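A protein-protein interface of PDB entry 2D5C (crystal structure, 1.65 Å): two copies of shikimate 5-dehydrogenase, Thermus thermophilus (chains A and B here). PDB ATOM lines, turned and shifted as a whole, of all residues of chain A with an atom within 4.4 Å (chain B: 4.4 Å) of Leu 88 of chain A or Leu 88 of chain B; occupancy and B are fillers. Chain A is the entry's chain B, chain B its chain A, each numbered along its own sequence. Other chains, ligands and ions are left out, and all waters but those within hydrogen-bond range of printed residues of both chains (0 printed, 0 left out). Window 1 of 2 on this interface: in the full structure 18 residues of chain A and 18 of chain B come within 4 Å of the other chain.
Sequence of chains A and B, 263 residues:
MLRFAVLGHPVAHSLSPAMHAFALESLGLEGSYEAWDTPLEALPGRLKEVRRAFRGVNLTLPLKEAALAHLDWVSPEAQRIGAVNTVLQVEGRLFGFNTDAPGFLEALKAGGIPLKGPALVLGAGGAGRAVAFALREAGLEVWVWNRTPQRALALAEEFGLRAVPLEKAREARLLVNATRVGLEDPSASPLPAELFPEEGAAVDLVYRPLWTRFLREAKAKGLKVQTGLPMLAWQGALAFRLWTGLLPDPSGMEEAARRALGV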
ATOM      1  N   ARG A  55     -18.767  36.265  -6.288  1.00  0.00           N
ATOM      2  CA  ARG A  55     -19.815  35.256  -6.384  1.00  0.00           C
ATOM      3  C   ARG A  55     -19.551  34.169  -5.349  1.00  0.00           C
ATOM      4  O   ARG A  55     -20.476  33.575  -4.779  1.00  0.00           O
ATOM      5  CB  ARG A  55     -19.825  34.649  -7.787  1.00  0.00           C
ATOM      6  CG  ARG A  55     -20.741  33.439  -7.938  1.00  0.00           C
ATOM      7  CD  ARG A  55     -22.210  33.751  -7.693  1.00  0.00           C
ATOM      8  NE  ARG A  55     -23.029  32.578  -8.005  1.00  0.00           N
ATOM      9  CZ  ARG A  55     -24.357  32.556  -8.022  1.00  0.00           C
ATOM     10  NH1 ARG A  55     -25.047  33.655  -7.732  1.00  0.00           N
ATOM     11  NH2 ARG A  55     -24.995  31.434  -8.357  1.00  0.00           N
ATOM     12  N   THR A  86     -15.909  26.687   1.702  1.00  0.00           N
ATOM     13  CA  THR A  86     -16.546  27.257   0.511  1.00  0.00           C
ATOM     14  C   THR A  86     -17.695  28.203   0.865  1.00  0.00           C
ATOM     15  O   THR A  86     -18.590  27.841   1.603  1.00  0.00           O
ATOM     16  CB  THR A  86     -17.064  26.126  -0.425  1.00  0.00           C
ATOM     17  OG1 THR A  86     -15.949  25.385  -0.932  1.00  0.00           O
ATOM     18  CG2 THR A  86     -17.826  26.688  -1.612  1.00  0.00           C
ATOM     19  N   VAL A  87     -17.643  29.429   0.348  1.00  0.00           N
ATOM     20  CA  VAL A  87     -18.691  30.415   0.598  1.00  0.00           C
ATOM     21  C   VAL A  87     -19.332  30.847  -0.717  1.00  0.00           C
ATOM     22  O   VAL A  87     -18.642  31.129  -1.696  1.00  0.00           O
ATOM     23  CB  VAL A  87     -18.130  31.675   1.291  1.00  0.00           C
ATOM     24  CG1 VAL A  87     -19.238  32.738   1.428  1.00  0.00           C
ATOM     25  CG2 VAL A  87     -17.564  31.306   2.655  1.00  0.00           C
ATOM     26  N   LEU A  88     -20.662  30.877  -0.730  1.00  0.00           N
ATOM     27  CA  LEU A  88     -21.437  31.299  -1.894  1.00  0.00           C
ATOM     28  C   LEU A  88     -22.100  32.618  -1.520  1.00  0.00           C
ATOM     29  O   LEU A  88     -22.588  32.771  -0.401  1.00  0.00           O
ATOM     30  CB  LEU A  88     -22.524  30.274  -2.215  1.00  0.00           C
ATOM     31  CG  LEU A  88     -23.683  30.756  -3.102  1.00  0.00           C
ATOM     32  CD1 LEU A  88     -23.189  30.931  -4.529  1.00  0.00           C
ATOM     33  CD2 LEU A  88     -24.829  29.729  -3.056  1.00  0.00           C
ATOM     34  N   GLN A  89     -22.119  33.564  -2.452  1.00  0.00           N
ATOM     35  CA  GLN A  89     -22.741  34.860  -2.199  1.00  0.00           C
ATOM     36  C   GLN A  89     -23.887  35.052  -3.176  1.00  0.00           C
ATOM     37  O   GLN A  89     -23.689  35.024  -4.394  1.00  0.00           O
ATOM     38  CB  GLN A  89     -21.716  35.999  -2.361  1.00  0.00           C
ATOM     39  CG  GLN A  89     -22.273  37.430  -2.187  1.00  0.00           C
ATOM     40  CD  GLN A  89     -22.925  37.984  -3.456  1.00  0.00           C
ATOM     41  OE1 GLN A  89     -24.142  38.176  -3.521  1.00  0.00           O
ATOM     42  NE2 GLN A  89     -22.113  38.234  -4.471  1.00  0.00           N
ATOM     43  N   VAL A  90     -25.087  35.229  -2.634  1.00  0.00           N
ATOM     44  CA  VAL A  90     -26.282  35.461  -3.442  1.00  0.00           C
ATOM     45  C   VAL A  90     -27.048  36.604  -2.772  1.00  0.00           C
ATOM     46  O   VAL A  90     -27.289  36.566  -1.563  1.00  0.00           O
ATOM     47  CB  VAL A  90     -27.169  34.201  -3.504  1.00  0.00           C
ATOM     48  CG1 VAL A  90     -28.469  34.517  -4.195  1.00  0.00           C
ATOM     49  CG2 VAL A  90     -26.450  33.092  -4.264  1.00  0.00           C
ATOM     50  N   ARG A  93     -26.009  37.883   0.535  1.00  0.00           N
ATOM     51  CA  ARG A  93     -26.069  36.971   1.679  1.00  0.00           C
ATOM     52  C   ARG A  93     -24.945  35.946   1.506  1.00  0.00           C
ATOM     53  O   ARG A  93     -24.584  35.618   0.377  1.00  0.00           O
ATOM     54  CB  ARG A  93     -27.407  36.229   1.705  1.00  0.00           C
ATOM     55  CG  ARG A  93     -28.630  37.110   1.508  1.00  0.00           C
ATOM     56  CD  ARG A  93     -28.737  38.188   2.566  1.00  0.00           C
ATOM     57  NE  ARG A  93     -29.900  39.041   2.315  1.00  0.00           N
ATOM     58  CZ  ARG A  93     -30.193  40.132   3.010  1.00  0.00           C
ATOM     59  NH1 ARG A  93     -29.404  40.512   4.007  1.00  0.00           N
ATOM     60  NH2 ARG A  93     -31.277  40.844   2.709  1.00  0.00           N
ATOM     61  N   LEU A  94     -24.408  35.432   2.610  1.00  0.00           N
ATOM     62  CA  LEU A  94     -23.320  34.446   2.538  1.00  0.00           C
ATOM     63  C   LEU A  94     -23.721  33.075   3.083  1.00  0.00           C
ATOM     64  O   LEU A  94     -24.240  32.955   4.197  1.00  0.00           O
ATOM     65  CB  LEU A  94     -22.082  34.955   3.300  1.00  0.00           C
ATOM     66  CG  LEU A  94     -21.411  36.281   2.884  1.00  0.00           C
ATOM     67  CD1 LEU A  94     -20.200  36.539   3.790  1.00  0.00           C
ATOM     68  CD2 LEU A  94     -20.978  36.237   1.422  1.00  0.00           C
ATOM     69  N   PHE A  95     -23.457  32.032   2.295  1.00  0.00           N
ATOM     70  CA  PHE A  95     -23.786  30.673   2.694  1.00  0.00           C
ATOM     71  C   PHE A  95     -22.492  29.864   2.758  1.00  0.00           C
ATOM     72  O   PHE A  95     -21.698  29.908   1.824  1.00  0.00           O
ATOM     73  CB  PHE A  95     -24.737  30.062   1.667  1.00  0.00           C
ATOM     74  CG  PHE A  95     -25.936  30.922   1.384  1.00  0.00           C
ATOM     75  CD1 PHE A  95     -25.846  31.992   0.501  1.00  0.00           C
ATOM     76  CD2 PHE A  95     -27.134  30.693   2.038  1.00  0.00           C
ATOM     77  CE1 PHE A  95     -26.935  32.825   0.276  1.00  0.00           C
ATOM     78  CE2 PHE A  95     -28.229  31.524   1.818  1.00  0.00           C
ATOM     79  CZ  PHE A  95     -28.127  32.582   0.939  1.00  0.00           C
ATOM     80  N   PHE A  97     -20.372  26.237   3.116  1.00  0.00           N
ATOM     81  CA  PHE A  97     -20.438  24.809   2.856  1.00  0.00           C
ATOM     82  C   PHE A  97     -19.060  24.202   3.086  1.00  0.00           C
ATOM     83  O   PHE A  97     -18.081  24.914   3.239  1.00  0.00           O
ATOM     84  CB  PHE A  97     -20.819  24.543   1.390  1.00  0.00           C
ATOM     85  CG  PHE A  97     -22.120  25.167   0.962  1.00  0.00           C
ATOM     86  CD1 PHE A  97     -22.164  26.495   0.555  1.00  0.00           C
ATOM     87  CD2 PHE A  97     -23.294  24.428   0.961  1.00  0.00           C
ATOM     88  CE1 PHE A  97     -23.378  27.080   0.150  1.00  0.00           C
ATOM     89  CE2 PHE A  97     -24.503  25.001   0.560  1.00  0.00           C
ATOM     90  CZ  PHE A  97     -24.539  26.331   0.154  1.00  0.00           C
ATOM     91  N   LEU A 242     -21.068  24.521  -6.903  1.00  0.00           N
ATOM     92  CA  LEU A 242     -21.921  25.170  -5.917  1.00  0.00           C
ATOM     93  C   LEU A 242     -22.134  26.609  -6.355  1.00  0.00           C
ATOM     94  O   LEU A 242     -23.234  27.153  -6.250  1.00  0.00           O
ATOM     95  CB  LEU A 242     -21.264  25.179  -4.531  1.00  0.00           C
ATOM     96  CG  LEU A 242     -21.560  24.079  -3.512  1.00  0.00           C
ATOM     97  CD1 LEU A 242     -20.723  24.327  -2.265  1.00  0.00           C
ATOM     98  CD2 LEU A 242     -23.044  24.069  -3.161  1.00  0.00           C
ATOM     99  N   TRP A 243     -21.076  27.232  -6.856  1.00  0.00           N
ATOM    100  CA  TRP A 243     -21.168  28.627  -7.271  1.00  0.00           C
ATOM    101  C   TRP A 243     -21.924  28.906  -8.557  1.00  0.00           C
ATOM    102  O   TRP A 243     -22.635  29.903  -8.646  1.00  0.00           O
ATOM    103  CB  TRP A 243     -19.773  29.249  -7.429  1.00  0.00           C
ATOM    104  CG  TRP A 243     -18.938  29.277  -6.189  1.00  0.00           C
ATOM    105  CD1 TRP A 243     -19.361  29.501  -4.918  1.00  0.00           C
ATOM    106  CD2 TRP A 243     -17.520  29.089  -6.116  1.00  0.00           C
ATOM    107  NE1 TRP A 243     -18.296  29.462  -4.046  1.00  0.00           N
ATOM    108  CE2 TRP A 243     -17.153  29.208  -4.758  1.00  0.00           C
ATOM    109  CE3 TRP A 243     -16.524  28.833  -7.068  1.00  0.00           C
ATOM    110  CZ2 TRP A 243     -15.833  29.072  -4.324  1.00  0.00           C
ATOM    111  CZ3 TRP A 243     -15.206  28.700  -6.638  1.00  0.00           C
ATOM    112  CH2 TRP A 243     -14.873  28.819  -5.272  1.00  0.00           C
ATOM    113  N   ARG B  55     -31.092  22.651 -10.730  1.00  0.00           N
ATOM    114  CA  ARG B  55     -30.216  23.660 -10.132  1.00  0.00           C
ATOM    115  C   ARG B  55     -31.083  24.755  -9.522  1.00  0.00           C
ATOM    116  O   ARG B  55     -30.706  25.382  -8.536  1.00  0.00           O
ATOM    117  CB  ARG B  55     -29.304  24.277 -11.189  1.00  0.00           C
ATOM    118  CG  ARG B  55     -28.610  25.560 -10.754  1.00  0.00           C
ATOM    119  CD  ARG B  55     -27.619  25.335  -9.616  1.00  0.00           C
ATOM    120  NE  ARG B  55     -26.806  26.526  -9.399  1.00  0.00           N
ATOM    121  CZ  ARG B  55     -25.796  26.603  -8.537  1.00  0.00           C
ATOM    122  NH1 ARG B  55     -25.462  25.547  -7.801  1.00  0.00           N
ATOM    123  NH2 ARG B  55     -25.123  27.741  -8.401  1.00  0.00           N
ATOM    124  N   THR B  86     -38.421  32.201  -6.595  1.00  0.00           N
ATOM    125  CA  THR B  86     -37.182  31.621  -7.099  1.00  0.00           C
ATOM    126  C   THR B  86     -36.513  30.748  -6.043  1.00  0.00           C
ATOM    127  O   THR B  86     -36.292  31.186  -4.910  1.00  0.00           O
ATOM    128  CB  THR B  86     -36.194  32.726  -7.523  1.00  0.00           C
ATOM    129  OG1 THR B  86     -36.801  33.543  -8.533  1.00  0.00           O
ATOM    130  CG2 THR B  86     -34.905  32.111  -8.085  1.00  0.00           C
ATOM    131  N   VAL B  87     -36.210  29.508  -6.421  1.00  0.00           N
ATOM    132  CA  VAL B  87     -35.552  28.570  -5.526  1.00  0.00           C
ATOM    133  C   VAL B  87     -34.230  28.110  -6.132  1.00  0.00           C
ATOM    134  O   VAL B  87     -34.171  27.773  -7.313  1.00  0.00           O
ATOM    135  CB  VAL B  87     -36.445  27.327  -5.265  1.00  0.00           C
ATOM    136  CG1 VAL B  87     -35.716  26.347  -4.343  1.00  0.00           C
ATOM    137  CG2 VAL B  87     -37.777  27.764  -4.655  1.00  0.00           C
ATOM    138  N   LEU B  88     -33.173  28.127  -5.317  1.00  0.00           N
ATOM    139  CA  LEU B  88     -31.832  27.681  -5.724  1.00  0.00           C
ATOM    140  C   LEU B  88     -31.535  26.376  -5.000  1.00  0.00           C
ATOM    141  O   LEU B  88     -31.780  26.274  -3.800  1.00  0.00           O
ATOM    142  CB  LEU B  88     -30.775  28.715  -5.320  1.00  0.00           C
ATOM    143  CG  LEU B  88     -29.310  28.272  -5.351  1.00  0.00           C
ATOM    144  CD1 LEU B  88     -28.911  27.934  -6.774  1.00  0.00           C
ATOM    145  CD2 LEU B  88     -28.410  29.388  -4.789  1.00  0.00           C
ATOM    146  N   GLN B  89     -31.018  25.379  -5.723  1.00  0.00           N
ATOM    147  CA  GLN B  89     -30.666  24.100  -5.112  1.00  0.00           C
ATOM    148  C   GLN B  89     -29.149  23.937  -5.066  1.00  0.00           C
ATOM    149  O   GLN B  89     -28.476  23.983  -6.105  1.00  0.00           O
ATOM    150  CB  GLN B  89     -31.301  22.930  -5.905  1.00  0.00           C
ATOM    151  CG  GLN B  89     -30.952  21.516  -5.382  1.00  0.00           C
ATOM    152  CD  GLN B  89     -29.609  20.994  -5.891  1.00  0.00           C
ATOM    153  OE1 GLN B  89     -28.699  20.709  -5.110  1.00  0.00           O
ATOM    154  NE2 GLN B  89     -29.482  20.872  -7.206  1.00  0.00           N
ATOM    155  N   VAL B  90     -28.617  23.770  -3.857  1.00  0.00           N
ATOM    156  CA  VAL B  90     -27.186  23.561  -3.651  1.00  0.00           C
ATOM    157  C   VAL B  90     -27.021  22.450  -2.606  1.00  0.00           C
ATOM    158  O   VAL B  90     -27.589  22.527  -1.517  1.00  0.00           O
ATOM    159  CB  VAL B  90     -26.480  24.847  -3.160  1.00  0.00           C
ATOM    160  CG1 VAL B  90     -26.367  25.861  -4.306  1.00  0.00           C
ATOM    161  CG2 VAL B  90     -27.247  25.443  -1.998  1.00  0.00           C
ATOM    162  N   ARG B  93     -29.956  21.193  -0.771  1.00  0.00           N
ATOM    163  CA  ARG B  93     -30.632  22.144   0.103  1.00  0.00           C
ATOM    164  C   ARG B  93     -31.355  23.143  -0.806  1.00  0.00           C
ATOM    165  O   ARG B  93     -30.907  23.412  -1.916  1.00  0.00           O
ATOM    166  CB  ARG B  93     -29.613  22.889   0.971  1.00  0.00           C
ATOM    167  CG  ARG B  93     -28.551  22.003   1.628  1.00  0.00           C
ATOM    168  CD  ARG B  93     -29.160  20.976   2.565  1.00  0.00           C
ATOM    169  NE  ARG B  93     -28.113  20.163   3.180  1.00  0.00           N
ATOM    170  CZ  ARG B  93     -28.340  19.205   4.072  1.00  0.00           C
ATOM    171  NH1 ARG B  93     -29.583  18.941   4.453  1.00  0.00           N
ATOM    172  NH2 ARG B  93     -27.324  18.519   4.586  1.00  0.00           N
ATOM    173  N   LEU B  94     -32.476  23.680  -0.338  1.00  0.00           N
ATOM    174  CA  LEU B  94     -33.244  24.632  -1.128  1.00  0.00           C
ATOM    175  C   LEU B  94     -33.262  25.995  -0.448  1.00  0.00           C
ATOM    176  O   LEU B  94     -33.593  26.097   0.735  1.00  0.00           O
ATOM    177  CB  LEU B  94     -34.685  24.133  -1.310  1.00  0.00           C
ATOM    178  CG  LEU B  94     -34.928  22.767  -1.969  1.00  0.00           C
ATOM    179  CD1 LEU B  94     -36.439  22.547  -2.089  1.00  0.00           C
ATOM    180  CD2 LEU B  94     -34.267  22.701  -3.358  1.00  0.00           C
ATOM    181  N   PHE B  95     -32.888  27.029  -1.201  1.00  0.00           N
ATOM    182  CA  PHE B  95     -32.856  28.416  -0.715  1.00  0.00           C
ATOM    183  C   PHE B  95     -33.924  29.216  -1.476  1.00  0.00           C
ATOM    184  O   PHE B  95     -33.973  29.167  -2.701  1.00  0.00           O
ATOM    185  CB  PHE B  95     -31.484  29.041  -0.993  1.00  0.00           C
ATOM    186  CG  PHE B  95     -30.350  28.413  -0.221  1.00  0.00           C
ATOM    187  CD1 PHE B  95     -29.033  28.624  -0.614  1.00  0.00           C
ATOM    188  CD2 PHE B  95     -30.591  27.641   0.910  1.00  0.00           C
ATOM    189  CE1 PHE B  95     -27.967  28.070   0.112  1.00  0.00           C
ATOM    190  CE2 PHE B  95     -29.533  27.085   1.639  1.00  0.00           C
ATOM    191  CZ  PHE B  95     -28.229  27.299   1.240  1.00  0.00           C
ATOM    192  N   PHE B  97     -35.891  32.792  -2.668  1.00  0.00           N
ATOM    193  CA  PHE B  97     -35.719  34.222  -2.880  1.00  0.00           C
ATOM    194  C   PHE B  97     -36.935  34.771  -3.592  1.00  0.00           C
ATOM    195  O   PHE B  97     -37.790  34.021  -4.054  1.00  0.00           O
ATOM    196  CB  PHE B  97     -34.510  34.514  -3.771  1.00  0.00           C
ATOM    197  CG  PHE B  97     -33.229  33.924  -3.281  1.00  0.00           C
ATOM    198  CD1 PHE B  97     -32.914  32.595  -3.536  1.00  0.00           C
ATOM    199  CD2 PHE B  97     -32.323  34.706  -2.569  1.00  0.00           C
ATOM    200  CE1 PHE B  97     -31.700  32.047  -3.091  1.00  0.00           C
ATOM    201  CE2 PHE B  97     -31.121  34.173  -2.123  1.00  0.00           C
ATOM    202  CZ  PHE B  97     -30.810  32.839  -2.387  1.00  0.00           C
ATOM    203  N   LEU B 242     -29.215  34.623  -9.944  1.00  0.00           N
ATOM    204  CA  LEU B 242     -29.132  33.963  -8.637  1.00  0.00           C
ATOM    205  C   LEU B 242     -28.630  32.537  -8.823  1.00  0.00           C
ATOM    206  O   LEU B 242     -27.784  32.063  -8.068  1.00  0.00           O
ATOM    207  CB  LEU B 242     -30.495  33.903  -7.937  1.00  0.00           C
ATOM    208  CG  LEU B 242     -31.126  35.204  -7.450  1.00  0.00           C
ATOM    209  CD1 LEU B 242     -32.436  34.890  -6.752  1.00  0.00           C
ATOM    210  CD2 LEU B 242     -30.182  35.921  -6.511  1.00  0.00           C
ATOM    211  N   TRP B 243     -29.154  31.849  -9.836  1.00  0.00           N
ATOM    212  CA  TRP B 243     -28.761  30.469 -10.087  1.00  0.00           C
ATOM    213  C   TRP B 243     -27.339  30.264 -10.605  1.00  0.00           C
ATOM    214  O   TRP B 243     -26.690  29.290 -10.240  1.00  0.00           O
ATOM    215  CB  TRP B 243     -29.705  29.811 -11.102  1.00  0.00           C
ATOM    216  CG  TRP B 243     -31.121  29.722 -10.670  1.00  0.00           C
ATOM    217  CD1 TRP B 243     -31.593  29.507  -9.397  1.00  0.00           C
ATOM    218  CD2 TRP B 243     -32.272  29.822 -11.515  1.00  0.00           C
ATOM    219  NE1 TRP B 243     -32.972  29.474  -9.406  1.00  0.00           N
ATOM    220  CE2 TRP B 243     -33.412  29.664 -10.692  1.00  0.00           C
ATOM    221  CE3 TRP B 243     -32.449  30.027 -12.894  1.00  0.00           C
ATOM    222  CZ2 TRP B 243     -34.715  29.710 -11.200  1.00  0.00           C
ATOM    223  CZ3 TRP B 243     -33.756  30.070 -13.403  1.00  0.00           C
ATOM    224  CH2 TRP B 243     -34.867  29.913 -12.555  1.00  0.00           C
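The backbone carbonyl oxygen (O) of Leu 242 of chain A lies within hydrogen-bond range of the guanidinium group (NH2) of Arg 55 of chain B (2.9 Å). NH2 of Arg 55 of chain B is in hydrogen-bond range of O of Trp 243 of chain A. The guanidinium group (NH2) of Arg 55 of chain A is in hydrogen-bond range of the backbone carbonyl oxygen (O) of Trp 243 of chain B. The backbone carbonyl oxygen (O) of Leu 242 of chain B is in hydrogen-bond range of the guanidinium group (NH2) of Arg 55 of chain A, at 2.9 Å.
The backbone carbonyl oxygen (O) of Thr 86 of chain B sits at hydrogen-bond distance from the backbone NH (N) of Phe 97 of chain B, at 2.8 Å. O of Arg 55 of chain B lies within hydrogen-bond range of N of Gln 89 of chain B (2.8 Å). O of Val 87 of chain B is in hydrogen-bond range of NE1 of Trp 243 of chain B (3.0 Å). The backbone carbonyl oxygen (O) of Leu 88 of chain B is in hydrogen-bond range of the backbone NH (N) of Phe 95 of chain B (2.9 Å). The backbone NH of Phe 97 of chain A lies within hydrogen-bond range of the backbone carbonyl oxygen of Thr 86 of chain A (2.8 Å). N of Gln 89 of chain A sits at hydrogen-bond distance from O of Arg 55 of chain A (2.8 Å).
Among the printed residues, merely in contact across the chains: Arg 55 of chain A with Arg 55 of chain B, Leu 88 of chain A with Leu 88 of chain B, Val 90 of chain A with Phe 97 of chain B, Val 90 of chain A with Leu 242 of chain B, Phe 95 of chain A with Phe 95 of chain B, Phe 97 of chain A with Val 90 of chain B, Phe 97 of chain A with Phe 95 of chain B and Leu 242 of chain A with Val 90 of chain B.
Printed residues of chain B within 4 Å of Leu 88 of chain A: Leu 88. Of the printed residues of chain A, Leu 88 of chain B touches Leu 88. Of the printed residues of chain A, Val 90 of chain B touches Phe 97 (3.6 Å) and Leu 242 (3.5 Å). Printed residues of chain B within 4 Å of Val 90 of chain A: Phe 97 and Leu 242. Printed residues of chain B within 4 Å of Phe 95 of chain A: Phe 95 (3.4 Å). Printed residues of chain A within 4 Å of Phe 95 of chain B: Phe 95 (3.4 Å) and Phe 97 (3.8 Å).
Of the 12 printed residues of chain A, 7 touch a printed residue of chain B. Along chain A the printed residues that touch a printed residue of chain B span positions 55 to 243. Among the printed residues, no Asp or Glu carboxylate lies within 4 Å of a Lys or Arg side-chain nitrogen of the other chain.
Arg 55 of chain A touches its own counterpart, Arg 55 of chain B. Arg 55 of chain A touches Leu 242 of chain B, and with the chains exchanged Leu 242 of chain A touches Arg 55 of chain B. Arg 55 of chain A touches Trp 243 of chain B, and with the chains exchanged Trp 243 of chain A touches Arg 55 of chain B. Val 90 of chain A touches Leu 242 of chain B, and with the chains exchanged Leu 242 of chain A touches Val 90 of chain B. Positions printed for both chains: 55, 86, 87, 88, 89, 90, 93, 94, 95, 97, 242 and 243.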
